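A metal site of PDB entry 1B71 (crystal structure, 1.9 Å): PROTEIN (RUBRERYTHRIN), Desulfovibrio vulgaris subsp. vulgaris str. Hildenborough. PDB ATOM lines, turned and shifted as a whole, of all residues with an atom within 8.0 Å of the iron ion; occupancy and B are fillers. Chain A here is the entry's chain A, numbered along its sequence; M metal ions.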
ATOM      1  N   ARG A 157      -1.782  19.248  30.283  1.00  0.00           N
ATOM      2  CA  ARG A 157      -1.969  20.686  30.118  1.00  0.00           C
ATOM      3  C   ARG A 157      -0.714  21.436  30.581  1.00  0.00           C
ATOM      4  O   ARG A 157      -0.141  21.144  31.626  1.00  0.00           O
ATOM      5  CB  ARG A 157      -3.220  21.154  30.869  1.00  0.00           C
ATOM      6  CG  ARG A 157      -3.708  22.541  30.459  1.00  0.00           C
ATOM      7  CD  ARG A 157      -4.693  23.074  31.471  1.00  0.00           C
ATOM      8  NE  ARG A 157      -4.112  23.118  32.818  1.00  0.00           N
ATOM      9  CZ  ARG A 157      -4.270  24.170  33.622  1.00  0.00           C
ATOM     10  NH1 ARG A 157      -4.972  25.210  33.185  1.00  0.00           N
ATOM     11  NH2 ARG A 157      -3.736  24.206  34.842  1.00  0.00           N
ATOM     12  N   CYS A 158      -0.326  22.392  29.749  1.00  0.00           N
ATOM     13  CA  CYS A 158       0.670  23.398  30.078  1.00  0.00           C
ATOM     14  C   CYS A 158       0.125  24.351  31.145  1.00  0.00           C
ATOM     15  O   CYS A 158      -0.854  25.072  30.968  1.00  0.00           O
ATOM     16  CB  CYS A 158       1.090  24.201  28.845  1.00  0.00           C
ATOM     17  SG  CYS A 158       2.332  25.446  29.236  1.00  0.00           S
ATOM     18  N   ARG A 159       0.795  24.337  32.296  1.00  0.00           N
ATOM     19  CA  ARG A 159       0.288  25.183  33.384  1.00  0.00           C
ATOM     20  C   ARG A 159       0.576  26.646  33.092  1.00  0.00           C
ATOM     21  O   ARG A 159      -0.100  27.546  33.586  1.00  0.00           O
ATOM     22  CB  ARG A 159       0.902  24.717  34.702  1.00  0.00           C
ATOM     23  CG  ARG A 159       0.577  23.246  34.968  1.00  0.00           C
ATOM     24  CD  ARG A 159       0.769  22.875  36.428  1.00  0.00           C
ATOM     25  NE  ARG A 159      -0.277  23.517  37.257  1.00  0.00           N
ATOM     26  CZ  ARG A 159       0.184  24.321  38.214  1.00  0.00           C
ATOM     27  NH1 ARG A 159       1.509  24.409  38.280  1.00  0.00           N
ATOM     28  NH2 ARG A 159      -0.619  24.967  39.036  1.00  0.00           N
ATOM     29  N   ASN A 160       1.610  26.856  32.278  1.00  0.00           N
ATOM     30  CA  ASN A 160       2.012  28.215  31.943  1.00  0.00           C
ATOM     31  C   ASN A 160       1.076  28.890  30.949  1.00  0.00           C
ATOM     32  O   ASN A 160       0.792  30.086  31.097  1.00  0.00           O
ATOM     33  CB  ASN A 160       3.458  28.223  31.403  1.00  0.00           C
ATOM     34  CG  ASN A 160       3.920  29.653  31.196  1.00  0.00           C
ATOM     35  OD1 ASN A 160       3.793  30.483  32.108  1.00  0.00           O
ATOM     36  ND2 ASN A 160       4.428  29.923  29.998  1.00  0.00           N
ATOM     37  N   CYS A 161       0.550  28.179  29.948  1.00  0.00           N
ATOM     38  CA  CYS A 161      -0.276  28.892  28.986  1.00  0.00           C
ATOM     39  C   CYS A 161      -1.553  28.160  28.615  1.00  0.00           C
ATOM     40  O   CYS A 161      -2.263  28.748  27.792  1.00  0.00           O
ATOM     41  CB  CYS A 161       0.483  29.122  27.682  1.00  0.00           C
ATOM     42  SG  CYS A 161       0.591  27.627  26.653  1.00  0.00           S
ATOM     43  N   GLY A 162      -1.843  26.991  29.172  1.00  0.00           N
ATOM     44  CA  GLY A 162      -3.117  26.325  28.963  1.00  0.00           C
ATOM     45  C   GLY A 162      -3.161  25.415  27.758  1.00  0.00           C
ATOM     46  O   GLY A 162      -4.172  24.801  27.390  1.00  0.00           O
ATOM     47  N   TYR A 163      -2.008  25.324  27.085  1.00  0.00           N
ATOM     48  CA  TYR A 163      -1.963  24.548  25.858  1.00  0.00           C
ATOM     49  C   TYR A 163      -2.282  23.098  26.199  1.00  0.00           C
ATOM     50  O   TYR A 163      -1.728  22.590  27.177  1.00  0.00           O
ATOM     51  CB  TYR A 163      -0.581  24.649  25.196  1.00  0.00           C
ATOM     52  CG  TYR A 163      -0.470  23.654  24.048  1.00  0.00           C
ATOM     53  CD1 TYR A 163      -1.087  23.939  22.831  1.00  0.00           C
ATOM     54  CD2 TYR A 163       0.225  22.465  24.175  1.00  0.00           C
ATOM     55  CE1 TYR A 163      -1.018  23.067  21.770  1.00  0.00           C
ATOM     56  CE2 TYR A 163       0.298  21.582  23.107  1.00  0.00           C
ATOM     57  CZ  TYR A 163      -0.320  21.895  21.915  1.00  0.00           C
ATOM     58  OH  TYR A 163      -0.244  21.028  20.866  1.00  0.00           O
ATOM     59  N   VAL A 164      -3.156  22.467  25.416  1.00  0.00           N
ATOM     60  CA  VAL A 164      -3.434  21.066  25.755  1.00  0.00           C
ATOM     61  C   VAL A 164      -2.862  20.111  24.726  1.00  0.00           C
ATOM     62  O   VAL A 164      -2.780  20.335  23.521  1.00  0.00           O
ATOM     63  CB  VAL A 164      -4.938  20.822  25.972  1.00  0.00           C
ATOM     64  CG1 VAL A 164      -5.202  19.369  26.308  1.00  0.00           C
ATOM     65  CG2 VAL A 164      -5.460  21.744  27.064  1.00  0.00           C
ATOM     66  N   PRO A 171       4.945  17.166  26.399  1.00  0.00           N
ATOM     67  CA  PRO A 171       5.961  17.509  25.401  1.00  0.00           C
ATOM     68  C   PRO A 171       7.206  18.103  26.057  1.00  0.00           C
ATOM     69  O   PRO A 171       7.129  18.626  27.170  1.00  0.00           O
ATOM     70  CB  PRO A 171       5.271  18.575  24.545  1.00  0.00           C
ATOM     71  CG  PRO A 171       4.340  19.248  25.502  1.00  0.00           C
ATOM     72  CD  PRO A 171       3.873  18.170  26.449  1.00  0.00           C
ATOM     73  N   LEU A 173       8.636  20.684  25.351  1.00  0.00           N
ATOM     74  CA  LEU A 173       8.472  22.120  25.190  1.00  0.00           C
ATOM     75  C   LEU A 173       7.055  22.425  24.747  1.00  0.00           C
ATOM     76  O   LEU A 173       6.463  21.778  23.882  1.00  0.00           O
ATOM     77  CB  LEU A 173       9.469  22.679  24.168  1.00  0.00           C
ATOM     78  CG  LEU A 173       9.961  24.116  24.393  1.00  0.00           C
ATOM     79  CD1 LEU A 173      11.230  24.155  25.228  1.00  0.00           C
ATOM     80  CD2 LEU A 173      10.189  24.824  23.068  1.00  0.00           C
ATOM     81  N   CYS A 174       6.492  23.458  25.381  1.00  0.00           N
ATOM     82  CA  CYS A 174       5.134  23.793  24.969  1.00  0.00           C
ATOM     83  C   CYS A 174       5.143  24.444  23.589  1.00  0.00           C
ATOM     84  O   CYS A 174       5.772  25.471  23.351  1.00  0.00           O
ATOM     85  CB  CYS A 174       4.456  24.709  25.999  1.00  0.00           C
ATOM     86  SG  CYS A 174       2.781  25.143  25.490  1.00  0.00           S
ATOM     87  N   PRO A 175       4.408  23.817  22.669  1.00  0.00           N
ATOM     88  CA  PRO A 175       4.245  24.392  21.335  1.00  0.00           C
ATOM     89  C   PRO A 175       3.694  25.802  21.423  1.00  0.00           C
ATOM     90  O   PRO A 175       3.977  26.609  20.531  1.00  0.00           O
ATOM     91  CB  PRO A 175       3.218  23.481  20.662  1.00  0.00           C
ATOM     92  CG  PRO A 175       3.228  22.208  21.441  1.00  0.00           C
ATOM     93  CD  PRO A 175       3.692  22.533  22.828  1.00  0.00           C
ATOM     94  N   ALA A 176       2.926  26.108  22.469  1.00  0.00           N
ATOM     95  CA  ALA A 176       2.290  27.425  22.551  1.00  0.00           C
ATOM     96  C   ALA A 176       3.205  28.457  23.205  1.00  0.00           C
ATOM     97  O   ALA A 176       3.576  29.444  22.571  1.00  0.00           O
ATOM     98  CB  ALA A 176       0.937  27.298  23.250  1.00  0.00           C
ATOM     99  N   CYS A 177       3.585  28.258  24.466  1.00  0.00           N
ATOM    100  CA  CYS A 177       4.386  29.247  25.189  1.00  0.00           C
ATOM    101  C   CYS A 177       5.864  28.943  25.211  1.00  0.00           C
ATOM    102  O   CYS A 177       6.669  29.740  25.714  1.00  0.00           O
ATOM    103  CB  CYS A 177       3.836  29.347  26.626  1.00  0.00           C
ATOM    104  SG  CYS A 177       4.261  27.914  27.651  1.00  0.00           S
ATOM    105  N   ALA A 178       6.302  27.805  24.677  1.00  0.00           N
ATOM    106  CA  ALA A 178       7.722  27.476  24.614  1.00  0.00           C
ATOM    107  C   ALA A 178       8.344  27.269  25.987  1.00  0.00           C
ATOM    108  O   ALA A 178       9.572  27.239  26.150  1.00  0.00           O
ATOM    109  CB  ALA A 178       8.467  28.566  23.846  1.00  0.00           C
ATOM    110  N   HIS A 179       7.533  27.088  27.023  1.00  0.00           N
ATOM    111  CA  HIS A 179       8.055  26.655  28.312  1.00  0.00           C
ATOM    112  C   HIS A 179       8.287  25.147  28.323  1.00  0.00           C
ATOM    113  O   HIS A 179       7.686  24.376  27.574  1.00  0.00           O
ATOM    114  CB  HIS A 179       7.085  27.095  29.414  1.00  0.00           C
ATOM    115  CG  HIS A 179       7.271  28.538  29.758  1.00  0.00           C
ATOM    116  ND1 HIS A 179       7.103  29.543  28.826  1.00  0.00           N
ATOM    117  CD2 HIS A 179       7.615  29.147  30.909  1.00  0.00           C
ATOM    118  CE1 HIS A 179       7.334  30.720  29.401  1.00  0.00           C
ATOM    119  NE2 HIS A 179       7.646  30.498  30.658  1.00  0.00           N
ATOM    120  N   PRO A 180       9.186  24.670  29.188  1.00  0.00           N
ATOM    121  CA  PRO A 180       9.564  23.257  29.212  1.00  0.00           C
ATOM    122  C   PRO A 180       8.566  22.337  29.887  1.00  0.00           C
ATOM    123  O   PRO A 180       7.614  22.745  30.555  1.00  0.00           O
ATOM    124  CB  PRO A 180      10.862  23.261  30.036  1.00  0.00           C
ATOM    125  CG  PRO A 180      10.862  24.528  30.824  1.00  0.00           C
ATOM    126  CD  PRO A 180       9.899  25.484  30.184  1.00  0.00           C
ATOM    127  N   HIS A 183       6.347  22.381  33.150  1.00  0.00           N
ATOM    128  CA  HIS A 183       5.087  23.094  33.370  1.00  0.00           C
ATOM    129  C   HIS A 183       3.859  22.252  33.051  1.00  0.00           C
ATOM    130  O   HIS A 183       2.736  22.718  33.273  1.00  0.00           O
ATOM    131  CB  HIS A 183       5.052  24.377  32.524  1.00  0.00           C
ATOM    132  CG  HIS A 183       6.175  25.288  32.913  1.00  0.00           C
ATOM    133  ND1 HIS A 183       5.973  26.435  33.635  1.00  0.00           N
ATOM    134  CD2 HIS A 183       7.503  25.200  32.666  1.00  0.00           C
ATOM    135  CE1 HIS A 183       7.141  27.034  33.820  1.00  0.00           C
ATOM    136  NE2 HIS A 183       8.092  26.306  33.249  1.00  0.00           N
ATOM    137  N   PHE A 184       4.064  21.052  32.540  1.00  0.00           N
ATOM    138  CA  PHE A 184       2.926  20.202  32.170  1.00  0.00           C
ATOM    139  C   PHE A 184       2.397  19.344  33.308  1.00  0.00           C
ATOM    140  O   PHE A 184       3.123  18.860  34.183  1.00  0.00           O
ATOM    141  CB  PHE A 184       3.333  19.282  30.998  1.00  0.00           C
ATOM    142  CG  PHE A 184       3.154  20.056  29.687  1.00  0.00           C
ATOM    143  CD1 PHE A 184       4.216  20.731  29.136  1.00  0.00           C
ATOM    144  CD2 PHE A 184       1.899  20.076  29.099  1.00  0.00           C
ATOM    145  CE1 PHE A 184       4.027  21.447  27.960  1.00  0.00           C
ATOM    146  CE2 PHE A 184       1.705  20.783  27.920  1.00  0.00           C
ATOM    147  CZ  PHE A 184       2.783  21.460  27.377  1.00  0.00           C
HETATM  148 FE    FE M   1       2.482  26.536  27.233  1.00  0.00          FE
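The iron ion is bound by SG of Cys 174 (2.3 Å), SG of Cys 161 (2.3 Å), SG of Cys 158 (2.3 Å) and SG of Cys 177 (2.3 Å). The iron ion has four donor atoms within binding distance.
A ring nitrogen (ND1) of His 179 sits at hydrogen-bond distance from the backbone carbonyl oxygen (O) of Cys 177, 3.1 Å away. The side-chain amide nitrogen (ND2) of Asn 160 lies close to the side-chain sulfur (SG) of Cys 177 (3.1 Å). The backbone carbonyl oxygen (O) of Tyr 163 is in hydrogen-bond range of the backbone NH (N) of Cys 158, 2.9 Å away. The side-chain sulfur of Cys 174 lies close to the backbone NH of Ala 176 (3.2 Å). N of Tyr 163 sits close to SG of Cys 161, 3.5 Å away. SG of Cys 158 sits close to N of Asn 160 (3.4 Å). N of Cys 174 sits at hydrogen-bond distance from O of His 179 (2.7 Å).
Four residues have an atom within 4 Å of the iron ion: Cys 158, Cys 161, Cys 174 and Cys 177.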
